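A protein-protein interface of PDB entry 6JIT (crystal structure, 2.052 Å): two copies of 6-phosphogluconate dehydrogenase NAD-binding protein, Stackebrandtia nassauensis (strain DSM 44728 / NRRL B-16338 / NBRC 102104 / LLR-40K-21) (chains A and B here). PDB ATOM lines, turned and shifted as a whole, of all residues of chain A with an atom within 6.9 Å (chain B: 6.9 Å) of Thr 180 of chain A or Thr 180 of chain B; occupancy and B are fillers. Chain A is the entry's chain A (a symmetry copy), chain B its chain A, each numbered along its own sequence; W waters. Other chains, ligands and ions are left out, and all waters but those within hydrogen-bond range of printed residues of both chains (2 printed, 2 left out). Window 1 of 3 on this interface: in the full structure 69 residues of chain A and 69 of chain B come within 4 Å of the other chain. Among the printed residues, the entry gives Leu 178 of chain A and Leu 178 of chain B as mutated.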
ATOM      1  N   LEU A 175     -10.291  -4.409   8.262  1.00  0.00           N
ATOM      2  CA  LEU A 175      -8.995  -4.414   8.937  1.00  0.00           C
ATOM      3  C   LEU A 175      -8.828  -3.195   9.834  1.00  0.00           C
ATOM      4  O   LEU A 175      -8.065  -3.239  10.806  1.00  0.00           O
ATOM      5  CB  LEU A 175      -7.865  -4.477   7.908  1.00  0.00           C
ATOM      6  CG  LEU A 175      -7.342  -5.858   7.499  1.00  0.00           C
ATOM      7  CD1 LEU A 175      -6.572  -6.502   8.651  1.00  0.00           C
ATOM      8  CD2 LEU A 175      -8.472  -6.765   7.049  1.00  0.00           C
ATOM      9  N   ASP A 176      -9.513  -2.098   9.505  1.00  0.00           N
ATOM     10  CA  ASP A 176      -9.581  -0.945  10.398  1.00  0.00           C
ATOM     11  C   ASP A 176     -10.112  -1.356  11.767  1.00  0.00           C
ATOM     12  O   ASP A 176      -9.537  -1.002  12.803  1.00  0.00           O
ATOM     13  CB  ASP A 176     -10.466   0.124   9.750  1.00  0.00           C
ATOM     14  CG  ASP A 176     -10.472   1.444  10.498  1.00  0.00           C
ATOM     15  OD1 ASP A 176      -9.735   1.602  11.492  1.00  0.00           O
ATOM     16  OD2 ASP A 176     -11.233   2.339  10.070  1.00  0.00           O
ATOM     17  N   VAL A 177     -11.204  -2.123  11.785  1.00  0.00           N
ATOM     18  CA  VAL A 177     -11.750  -2.633  13.040  1.00  0.00           C
ATOM     19  C   VAL A 177     -10.760  -3.583  13.705  1.00  0.00           C
ATOM     20  O   VAL A 177     -10.464  -3.459  14.900  1.00  0.00           O
ATOM     21  CB  VAL A 177     -13.105  -3.322  12.790  1.00  0.00           C
ATOM     22  CG1 VAL A 177     -13.640  -3.942  14.077  1.00  0.00           C
ATOM     23  CG2 VAL A 177     -14.108  -2.339  12.203  1.00  0.00           C
ATOM     24  N   LEU A 178     -10.227  -4.539  12.939  1.00  0.00           N
ATOM     25  CA  LEU A 178      -9.355  -5.563  13.512  1.00  0.00           C
ATOM     26  C   LEU A 178      -8.099  -4.953  14.122  1.00  0.00           C
ATOM     27  O   LEU A 178      -7.774  -5.211  15.287  1.00  0.00           O
ATOM     28  CB  LEU A 178      -8.983  -6.595  12.445  1.00  0.00           C
ATOM     29  CG  LEU A 178      -7.928  -7.625  12.862  1.00  0.00           C
ATOM     30  CD1 LEU A 178      -8.465  -8.545  13.947  1.00  0.00           C
ATOM     31  CD2 LEU A 178      -7.434  -8.438  11.668  1.00  0.00           C
ATOM     32  N   LEU A 179      -7.379  -4.136  13.349  1.00  0.00           N
ATOM     33  CA  LEU A 179      -6.103  -3.601  13.819  1.00  0.00           C
ATOM     34  C   LEU A 179      -6.291  -2.649  14.995  1.00  0.00           C
ATOM     35  O   LEU A 179      -5.499  -2.666  15.945  1.00  0.00           O
ATOM     36  CB  LEU A 179      -5.373  -2.892  12.679  1.00  0.00           C
ATOM     37  CG  LEU A 179      -4.928  -3.733  11.481  1.00  0.00           C
ATOM     38  CD1 LEU A 179      -3.915  -2.964  10.635  1.00  0.00           C
ATOM     39  CD2 LEU A 179      -4.362  -5.066  11.931  1.00  0.00           C
ATOM     40  N   THR A 180      -7.315  -1.797  14.943  1.00  0.00           N
ATOM     41  CA  THR A 180      -7.549  -0.867  16.044  1.00  0.00           C
ATOM     42  C   THR A 180      -7.958  -1.610  17.310  1.00  0.00           C
ATOM     43  O   THR A 180      -7.478  -1.290  18.403  1.00  0.00           O
ATOM     44  CB  THR A 180      -8.616   0.158  15.655  1.00  0.00           C
ATOM     45  OG1 THR A 180      -8.274   0.753  14.396  1.00  0.00           O
ATOM     46  CG2 THR A 180      -8.720   1.257  16.714  1.00  0.00           C
ATOM     47  N   THR A 181      -8.835  -2.609  17.176  1.00  0.00           N
ATOM     48  CA  THR A 181      -9.250  -3.403  18.329  1.00  0.00           C
ATOM     49  C   THR A 181      -8.072  -4.151  18.942  1.00  0.00           C
ATOM     50  O   THR A 181      -7.910  -4.163  20.169  1.00  0.00           O
ATOM     51  CB  THR A 181     -10.352  -4.381  17.924  1.00  0.00           C
ATOM     52  OG1 THR A 181     -11.493  -3.649  17.459  1.00  0.00           O
ATOM     53  CG2 THR A 181     -10.755  -5.259  19.104  1.00  0.00           C
ATOM     54  N   LEU A 182      -7.235  -4.774  18.105  1.00  0.00           N
ATOM     55  CA  LEU A 182      -6.062  -5.477  18.621  1.00  0.00           C
ATOM     56  C   LEU A 182      -5.114  -4.520  19.330  1.00  0.00           C
ATOM     57  O   LEU A 182      -4.547  -4.859  20.375  1.00  0.00           O
ATOM     58  CB  LEU A 182      -5.338  -6.214  17.491  1.00  0.00           C
ATOM     59  CG  LEU A 182      -6.053  -7.421  16.869  1.00  0.00           C
ATOM     60  CD1 LEU A 182      -5.153  -8.126  15.856  1.00  0.00           C
ATOM     61  CD2 LEU A 182      -6.523  -8.395  17.941  1.00  0.00           C
ATOM     62  N   ALA A 183      -4.928  -3.317  18.777  1.00  0.00           N
ATOM     63  CA  ALA A 183      -4.079  -2.326  19.432  1.00  0.00           C
ATOM     64  C   ALA A 183      -4.619  -1.957  20.810  1.00  0.00           C
ATOM     65  O   ALA A 183      -3.844  -1.720  21.744  1.00  0.00           O
ATOM     66  CB  ALA A 183      -3.956  -1.076  18.563  1.00  0.00           C
ATOM     67  N   SER A 184      -5.945  -1.893  20.955  1.00  0.00           N
ATOM     68  CA  SER A 184      -6.518  -1.518  22.241  1.00  0.00           C
ATOM     69  C   SER A 184      -6.309  -2.607  23.285  1.00  0.00           C
ATOM     70  O   SER A 184      -6.183  -2.303  24.477  1.00  0.00           O
ATOM     71  CB  SER A 184      -8.006  -1.203  22.090  1.00  0.00           C
ATOM     72  OG  SER A 184      -8.777  -2.385  21.994  1.00  0.00           O
ATOM     73  N   VAL A 185      -6.264  -3.871  22.859  1.00  0.00           N
ATOM     74  CA  VAL A 185      -5.995  -4.963  23.790  1.00  0.00           C
ATOM     75  C   VAL A 185      -4.563  -4.885  24.302  1.00  0.00           C
ATOM     76  O   VAL A 185      -4.301  -5.075  25.495  1.00  0.00           O
ATOM     77  CB  VAL A 185      -6.282  -6.318  23.119  1.00  0.00           C
ATOM     78  CG1 VAL A 185      -5.914  -7.464  24.049  1.00  0.00           C
ATOM     79  CG2 VAL A 185      -7.737  -6.402  22.727  1.00  0.00           C
ATOM     80  N   HIS A 187      -2.752  -2.130  24.372  1.00  0.00           N
ATOM     81  CA  HIS A 187      -2.637  -0.912  25.166  1.00  0.00           C
ATOM     82  C   HIS A 187      -3.250  -1.088  26.552  1.00  0.00           C
ATOM     83  O   HIS A 187      -2.662  -0.663  27.555  1.00  0.00           O
ATOM     84  CB  HIS A 187      -3.288   0.259  24.431  1.00  0.00           C
ATOM     85  CG  HIS A 187      -3.022   1.592  25.064  1.00  0.00           C
ATOM     86  ND1 HIS A 187      -3.835   2.126  26.041  1.00  0.00           N
ATOM     87  CD2 HIS A 187      -2.033   2.495  24.862  1.00  0.00           C
ATOM     88  CE1 HIS A 187      -3.357   3.301  26.414  1.00  0.00           C
ATOM     89  NE2 HIS A 187      -2.265   3.547  25.714  1.00  0.00           N
ATOM     90  N   ILE A 253      -8.889   7.633  30.882  1.00  0.00           N
ATOM     91  CA  ILE A 253      -7.952   6.677  30.296  1.00  0.00           C
ATOM     92  C   ILE A 253      -6.654   7.376  29.912  1.00  0.00           C
ATOM     93  O   ILE A 253      -5.557   6.846  30.133  1.00  0.00           O
ATOM     94  CB  ILE A 253      -8.601   5.969  29.091  1.00  0.00           C
ATOM     95  CG1 ILE A 253      -9.797   5.126  29.545  1.00  0.00           C
ATOM     96  CG2 ILE A 253      -7.580   5.106  28.356  1.00  0.00           C
ATOM     97  CD1 ILE A 253     -10.696   4.675  28.407  1.00  0.00           C
ATOM     98  N   LEU A 266      -2.821   6.328  21.102  1.00  0.00           N
ATOM     99  CA  LEU A 266      -4.101   5.658  20.876  1.00  0.00           C
ATOM    100  C   LEU A 266      -5.216   6.252  21.730  1.00  0.00           C
ATOM    101  O   LEU A 266      -6.244   6.662  21.163  1.00  0.00           O
ATOM    102  CB  LEU A 266      -3.945   4.149  21.096  1.00  0.00           C
ATOM    103  CG  LEU A 266      -5.138   3.283  20.696  1.00  0.00           C
ATOM    104  CD1 LEU A 266      -5.378   3.407  19.202  1.00  0.00           C
ATOM    105  CD2 LEU A 266      -4.892   1.834  21.078  1.00  0.00           C
ATOM    106  N   PRO A 267      -5.100   6.340  23.065  1.00  0.00           N
ATOM    107  CA  PRO A 267      -6.195   6.948  23.838  1.00  0.00           C
ATOM    108  C   PRO A 267      -6.386   8.431  23.565  1.00  0.00           C
ATOM    109  O   PRO A 267      -7.507   8.930  23.704  1.00  0.00           O
ATOM    110  CB  PRO A 267      -5.781   6.694  25.295  1.00  0.00           C
ATOM    111  CG  PRO A 267      -4.303   6.553  25.244  1.00  0.00           C
ATOM    112  CD  PRO A 267      -4.023   5.853  23.948  1.00  0.00           C
ATOM    113  N   VAL A 270      -8.853   8.618  20.719  1.00  0.00           N
ATOM    114  CA  VAL A 270     -10.225   8.452  21.191  1.00  0.00           C
ATOM    115  C   VAL A 270     -10.692   9.705  21.922  1.00  0.00           C
ATOM    116  O   VAL A 270     -11.827  10.162  21.738  1.00  0.00           O
ATOM    117  CB  VAL A 270     -10.336   7.202  22.086  1.00  0.00           C
ATOM    118  CG1 VAL A 270     -11.730   7.101  22.694  1.00  0.00           C
ATOM    119  CG2 VAL A 270     -10.005   5.940  21.298  1.00  0.00           C
ATOM    120  N   TYR A 274     -13.975  12.351  21.037  1.00  0.00           N
ATOM    121  CA  TYR A 274     -15.030  12.773  21.951  1.00  0.00           C
ATOM    122  C   TYR A 274     -14.952  14.266  22.242  1.00  0.00           C
ATOM    123  O   TYR A 274     -15.989  14.926  22.370  1.00  0.00           O
ATOM    124  CB  TYR A 274     -14.965  11.960  23.241  1.00  0.00           C
ATOM    125  CG  TYR A 274     -15.577  10.589  23.095  1.00  0.00           C
ATOM    126  CD1 TYR A 274     -16.946  10.443  22.930  1.00  0.00           C
ATOM    127  CD2 TYR A 274     -14.789   9.444  23.113  1.00  0.00           C
ATOM    128  CE1 TYR A 274     -17.518   9.201  22.784  1.00  0.00           C
ATOM    129  CE2 TYR A 274     -15.355   8.189  22.976  1.00  0.00           C
ATOM    130  CZ  TYR A 274     -16.723   8.076  22.815  1.00  0.00           C
ATOM    131  OH  TYR A 274     -17.306   6.838  22.675  1.00  0.00           O
ATOM    132  N   LEU B 175     -12.479  -0.284  29.724  1.00  0.00           N
ATOM    133  CA  LEU B 175     -13.124   0.749  28.917  1.00  0.00           C
ATOM    134  C   LEU B 175     -12.211   1.239  27.802  1.00  0.00           C
ATOM    135  O   LEU B 175     -12.694   1.726  26.773  1.00  0.00           O
ATOM    136  CB  LEU B 175     -13.556   1.918  29.805  1.00  0.00           C
ATOM    137  CG  LEU B 175     -14.970   1.889  30.393  1.00  0.00           C
ATOM    138  CD1 LEU B 175     -16.012   2.103  29.297  1.00  0.00           C
ATOM    139  CD2 LEU B 175     -15.236   0.587  31.125  1.00  0.00           C
ATOM    140  N   ASP B 176     -10.896   1.139  28.002  1.00  0.00           N
ATOM    141  CA  ASP B 176      -9.939   1.393  26.931  1.00  0.00           C
ATOM    142  C   ASP B 176     -10.230   0.503  25.727  1.00  0.00           C
ATOM    143  O   ASP B 176     -10.282   0.975  24.586  1.00  0.00           O
ATOM    144  CB  ASP B 176      -8.524   1.160  27.471  1.00  0.00           C
ATOM    145  CG  ASP B 176      -7.428   1.564  26.503  1.00  0.00           C
ATOM    146  OD1 ASP B 176      -7.723   2.108  25.419  1.00  0.00           O
ATOM    147  OD2 ASP B 176      -6.250   1.331  26.847  1.00  0.00           O
ATOM    148  N   VAL B 177     -10.442  -0.792  25.973  1.00  0.00           N
ATOM    149  CA  VAL B 177     -10.803  -1.717  24.902  1.00  0.00           C
ATOM    150  C   VAL B 177     -12.158  -1.345  24.310  1.00  0.00           C
ATOM    151  O   VAL B 177     -12.312  -1.245  23.087  1.00  0.00           O
ATOM    152  CB  VAL B 177     -10.800  -3.166  25.425  1.00  0.00           C
ATOM    153  CG1 VAL B 177     -11.266  -4.131  24.340  1.00  0.00           C
ATOM    154  CG2 VAL B 177      -9.417  -3.550  25.935  1.00  0.00           C
ATOM    155  N   LEU B 178     -13.156  -1.125  25.170  1.00  0.00           N
ATOM    156  CA  LEU B 178     -14.516  -0.872  24.696  1.00  0.00           C
ATOM    157  C   LEU B 178     -14.587   0.391  23.846  1.00  0.00           C
ATOM    158  O   LEU B 178     -15.093   0.365  22.718  1.00  0.00           O
ATOM    159  CB  LEU B 178     -15.477  -0.773  25.882  1.00  0.00           C
ATOM    160  CG  LEU B 178     -16.904  -0.331  25.540  1.00  0.00           C
ATOM    161  CD1 LEU B 178     -17.615  -1.385  24.708  1.00  0.00           C
ATOM    162  CD2 LEU B 178     -17.709  -0.009  26.797  1.00  0.00           C
ATOM    163  N   LEU B 179     -14.083   1.511  24.372  1.00  0.00           N
ATOM    164  CA  LEU B 179     -14.215   2.786  23.671  1.00  0.00           C
ATOM    165  C   LEU B 179     -13.417   2.799  22.371  1.00  0.00           C
ATOM    166  O   LEU B 179     -13.886   3.328  21.356  1.00  0.00           O
ATOM    167  CB  LEU B 179     -13.770   3.936  24.573  1.00  0.00           C
ATOM    168  CG  LEU B 179     -14.578   4.203  25.845  1.00  0.00           C
ATOM    169  CD1 LEU B 179     -14.236   5.577  26.417  1.00  0.00           C
ATOM    170  CD2 LEU B 179     -16.066   4.077  25.580  1.00  0.00           C
ATOM    171  N   THR B 180     -12.204   2.244  22.385  1.00  0.00           N
ATOM    172  CA  THR B 180     -11.398   2.221  21.169  1.00  0.00           C
ATOM    173  C   THR B 180     -12.027   1.321  20.112  1.00  0.00           C
ATOM    174  O   THR B 180     -12.076   1.684  18.932  1.00  0.00           O
ATOM    175  CB  THR B 180      -9.974   1.761  21.486  1.00  0.00           C
ATOM    176  OG1 THR B 180      -9.448   2.539  22.569  1.00  0.00           O
ATOM    177  CG2 THR B 180      -9.068   1.930  20.265  1.00  0.00           C
ATOM    178  N   THR B 181     -12.523   0.149  20.524  1.00  0.00           N
ATOM    179  CA  THR B 181     -13.182  -0.756  19.588  1.00  0.00           C
ATOM    180  C   THR B 181     -14.433  -0.123  18.990  1.00  0.00           C
ATOM    181  O   THR B 181     -14.654  -0.205  17.774  1.00  0.00           O
ATOM    182  CB  THR B 181     -13.529  -2.070  20.286  1.00  0.00           C
ATOM    183  OG1 THR B 181     -12.326  -2.704  20.738  1.00  0.00           O
ATOM    184  CG2 THR B 181     -14.273  -3.006  19.337  1.00  0.00           C
ATOM    185  N   LEU B 182     -15.259   0.518  19.824  1.00  0.00           N
ATOM    186  CA  LEU B 182     -16.456   1.182  19.313  1.00  0.00           C
ATOM    187  C   LEU B 182     -16.095   2.295  18.340  1.00  0.00           C
ATOM    188  O   LEU B 182     -16.764   2.474  17.315  1.00  0.00           O
ATOM    189  CB  LEU B 182     -17.300   1.728  20.467  1.00  0.00           C
ATOM    190  CG  LEU B 182     -17.996   0.704  21.374  1.00  0.00           C
ATOM    191  CD1 LEU B 182     -18.901   1.400  22.389  1.00  0.00           C
ATOM    192  CD2 LEU B 182     -18.783  -0.310  20.557  1.00  0.00           C
ATOM    193  N   ALA B 183     -15.039   3.057  18.642  1.00  0.00           N
ATOM    194  CA  ALA B 183     -14.598   4.106  17.726  1.00  0.00           C
ATOM    195  C   ALA B 183     -14.191   3.528  16.375  1.00  0.00           C
ATOM    196  O   ALA B 183     -14.423   4.149  15.331  1.00  0.00           O
ATOM    197  CB  ALA B 183     -13.436   4.889  18.335  1.00  0.00           C
ATOM    198  N   SER B 184     -13.573   2.343  16.374  1.00  0.00           N
ATOM    199  CA  SER B 184     -13.134   1.755  15.114  1.00  0.00           C
ATOM    200  C   SER B 184     -14.317   1.305  14.267  1.00  0.00           C
ATOM    201  O   SER B 184     -14.237   1.327  13.034  1.00  0.00           O
ATOM    202  CB  SER B 184     -12.188   0.583  15.375  1.00  0.00           C
ATOM    203  OG  SER B 184     -12.897  -0.576  15.770  1.00  0.00           O
ATOM    204  N   VAL B 185     -15.417   0.900  14.906  1.00  0.00           N
ATOM    205  CA  VAL B 185     -16.615   0.522  14.162  1.00  0.00           C
ATOM    206  C   VAL B 185     -17.228   1.740  13.486  1.00  0.00           C
ATOM    207  O   VAL B 185     -17.648   1.680  12.324  1.00  0.00           O
ATOM    208  CB  VAL B 185     -17.624  -0.173  15.095  1.00  0.00           C
ATOM    209  CG1 VAL B 185     -18.913  -0.484  14.352  1.00  0.00           C
ATOM    210  CG2 VAL B 185     -17.021  -1.436  15.660  1.00  0.00           C
ATOM    211  N   HIS B 187     -15.565   4.480  12.713  1.00  0.00           N
ATOM    212  CA  HIS B 187     -14.618   4.943  11.704  1.00  0.00           C
ATOM    213  C   HIS B 187     -14.667   4.072  10.452  1.00  0.00           C
ATOM    214  O   HIS B 187     -14.657   4.591   9.328  1.00  0.00           O
ATOM    215  CB  HIS B 187     -13.204   4.976  12.285  1.00  0.00           C
ATOM    216  CG  HIS B 187     -12.203   5.649  11.397  1.00  0.00           C
ATOM    217  ND1 HIS B 187     -11.483   4.968  10.438  1.00  0.00           N
ATOM    218  CD2 HIS B 187     -11.804   6.941  11.318  1.00  0.00           C
ATOM    219  CE1 HIS B 187     -10.684   5.812   9.807  1.00  0.00           C
ATOM    220  NE2 HIS B 187     -10.860   7.016  10.322  1.00  0.00           N
ATOM    221  N   ILE B 253      -4.917   1.853   5.292  1.00  0.00           N
ATOM    222  CA  ILE B 253      -6.111   2.401   5.930  1.00  0.00           C
ATOM    223  C   ILE B 253      -6.010   3.918   6.031  1.00  0.00           C
ATOM    224  O   ILE B 253      -6.986   4.639   5.786  1.00  0.00           O
ATOM    225  CB  ILE B 253      -6.323   1.747   7.309  1.00  0.00           C
ATOM    226  CG1 ILE B 253      -6.607   0.250   7.154  1.00  0.00           C
ATOM    227  CG2 ILE B 253      -7.455   2.435   8.066  1.00  0.00           C
ATOM    228  CD1 ILE B 253      -6.488  -0.534   8.449  1.00  0.00           C
ATOM    229  N   LEU B 266      -7.610   8.497  14.390  1.00  0.00           N
ATOM    230  CA  LEU B 266      -7.624   7.119  14.878  1.00  0.00           C
ATOM    231  C   LEU B 266      -6.706   6.214  14.063  1.00  0.00           C
ATOM    232  O   LEU B 266      -5.827   5.568  14.661  1.00  0.00           O
ATOM    233  CB  LEU B 266      -9.065   6.596  14.917  1.00  0.00           C
ATOM    234  CG  LEU B 266      -9.273   5.246  15.601  1.00  0.00           C
ATOM    235  CD1 LEU B 266      -8.887   5.352  17.064  1.00  0.00           C
ATOM    236  CD2 LEU B 266     -10.717   4.799  15.461  1.00  0.00           C
ATOM    237  N   PRO B 267      -6.830   6.114  12.731  1.00  0.00           N
ATOM    238  CA  PRO B 267      -5.898   5.247  11.989  1.00  0.00           C
ATOM    239  C   PRO B 267      -4.460   5.738  12.012  1.00  0.00           C
ATOM    240  O   PRO B 267      -3.541   4.917  11.912  1.00  0.00           O
ATOM    241  CB  PRO B 267      -6.472   5.249  10.566  1.00  0.00           C
ATOM    242  CG  PRO B 267      -7.235   6.520  10.472  1.00  0.00           C
ATOM    243  CD  PRO B 267      -7.835   6.715  11.832  1.00  0.00           C
ATOM    244  N   VAL B 270      -2.893   4.125  15.038  1.00  0.00           N
ATOM    245  CA  VAL B 270      -2.499   2.746  14.764  1.00  0.00           C
ATOM    246  C   VAL B 270      -1.260   2.714  13.877  1.00  0.00           C
ATOM    247  O   VAL B 270      -0.336   1.923  14.104  1.00  0.00           O
ATOM    248  CB  VAL B 270      -3.668   1.970  14.128  1.00  0.00           C
ATOM    249  CG1 VAL B 270      -3.220   0.574  13.711  1.00  0.00           C
ATOM    250  CG2 VAL B 270      -4.849   1.887  15.088  1.00  0.00           C
ATOM    251  N   TYR B 274       2.634   1.034  14.639  1.00  0.00           N
ATOM    252  CA  TYR B 274       3.366   0.101  13.790  1.00  0.00           C
ATOM    253  C   TYR B 274       4.633   0.734  13.228  1.00  0.00           C
ATOM    254  O   TYR B 274       5.659   0.057  13.101  1.00  0.00           O
ATOM    255  CB  TYR B 274       2.464  -0.409  12.669  1.00  0.00           C
ATOM    256  CG  TYR B 274       1.523  -1.495  13.128  1.00  0.00           C
ATOM    257  CD1 TYR B 274       2.008  -2.748  13.472  1.00  0.00           C
ATOM    258  CD2 TYR B 274       0.156  -1.267  13.229  1.00  0.00           C
ATOM    259  CE1 TYR B 274       1.165  -3.744  13.905  1.00  0.00           C
ATOM    260  CE2 TYR B 274      -0.702  -2.264  13.653  1.00  0.00           C
ATOM    261  CZ  TYR B 274      -0.189  -3.504  13.987  1.00  0.00           C
ATOM    262  OH  TYR B 274      -1.025  -4.511  14.414  1.00  0.00           O
HETATM  263  O   HOH W   1      -2.968  -3.722  15.885  1.00  0.00           O
HETATM  264  O   HOH W   2     -15.924   5.162  21.317  1.00  0.00           O
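Water W1 lies within hydrogen-bond range of OH of Tyr 274 of chain B (2.6 Å) and O of Leu 179 of chain A (2.7 Å). Water W2 bridges the side-chain hydroxyl (OH) of Tyr 274 of chain A and the backbone carbonyl oxygen (O) of Leu 179 of chain B.
Leu 175 of chain A touches Ile 253 of chain B, and with the chains exchanged Ile 253 of chain A touches Leu 175 of chain B. Asp 176 of chain A touches Ile 253 of chain B, and with the chains exchanged Ile 253 of chain A touches Asp 176 of chain B. Val 177 of chain A touches Ser 184 of chain B, and with the chains exchanged Ser 184 of chain A touches Val 177 of chain B. Thr 180 of chain A touches Ser 184 of chain B, and with the chains exchanged Ser 184 of chain A touches Thr 180 of chain B. Positions printed for both chains: 175, 176, 177, 178, 179, 180, 181, 182, 183, 184, 185, 187, 253, 266, 267, 270 and 274. Of the 16 pairs that touch across the chains among the printed residues, 16 have their exchanged pair printed and touching as well.
The backbone carbonyl oxygen of Val 177 of chain A sits at hydrogen-bond distance from the side-chain hydroxyl of Thr 181 of chain A, 2.8 Å away. The backbone carbonyl oxygen (O) of Val 177 of chain B sits at hydrogen-bond distance from the side-chain hydroxyl (OG1) of Thr 181 of chain B, at 2.8 Å. The backbone carbonyl oxygen (O) of Asp 176 of chain A is in hydrogen-bond range of the side-chain hydroxyl (OG1) of Thr 180 of chain A (2.7 Å). The side-chain hydroxyl of Ser 184 of chain B lies within hydrogen-bond range of the backbone carbonyl oxygen of Thr 181 of chain B (2.7 Å). The side-chain hydroxyl of Thr 180 of chain B lies within hydrogen-bond range of the backbone carbonyl oxygen of Asp 176 of chain B, at 2.7 Å. The backbone carbonyl oxygen of Thr 181 of chain A is in hydrogen-bond range of the side-chain hydroxyl of Ser 184 of chain A, at 2.7 Å.
Thr 180 of chain A touches three residues of chain B. Of chain A, only Thr 180 (3.6 Å), Ser 184 (3.6 Å) and Val 270 (3.7 Å) come within 4 Å of Thr 180 of chain B. Of the printed residues of chain A, Asp 176 of chain B touches His 187 (2.7 Å) and Ile 253 (3.6 Å). Printed residues of chain A within 4 Å of Leu 175 of chain B: Ile 253 (3.8 Å). Tyr 274 of chain A touches none of the printed residues of chain B. Pro 267 of chain B touches none of the printed residues of chain A. The nearest residue of chain A that does not touch Thr 180 of chain B is Leu 266 of chain A (4.1 Å). The nearest printed residue of chain B that does not touch Thr 181 of chain A is Val 177 of chain B (5.4 Å).
Among the printed residues, 16 pairs touch across the chains. Among the printed residues, no Asp or Glu carboxylate lies within 4 Å of a Lys or Arg side-chain nitrogen of the other chain.
Among the printed residues, pairs that only touch across the chains: Leu 175 of chain A with Ile 253 of chain B (3.8 Å), Asp 176 of chain A with Ile 253 of chain B (3.6 Å), Val 177 of chain A with Ser 184 of chain B (3.6 Å), Thr 180 of chain A with Thr 180 of chain B (3.6 Å), Thr 180 of chain A with Ser 184 of chain B (3.6 Å), Thr 180 of chain A with Val 270 of chain B (3.7 Å), Thr 181 of chain A with Thr 181 of chain B (3.4 Å), Thr 181 of chain A with Ser 184 of chain B (3.8 Å), Ser 184 of chain A with Val 177 of chain B (3.6 Å), Ser 184 of chain A with Thr 180 of chain B (3.6 Å), Ser 184 of chain A with Thr 181 of chain B (3.8 Å), Ile 253 of chain A with Leu 175 of chain B (3.8 Å), Ile 253 of chain A with Asp 176 of chain B (3.6 Å) and Val 270 of chain A with Thr 180 of chain B (3.7 Å).
A ring nitrogen (ND1) of His 187 of chain A sits at hydrogen-bond distance from the side-chain carboxylate of Asp 176 of chain B, at 2.7 Å. ND1 of His 187 of chain B sits at hydrogen-bond distance from OD2 of Asp 176 of chain A (2.7 Å).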
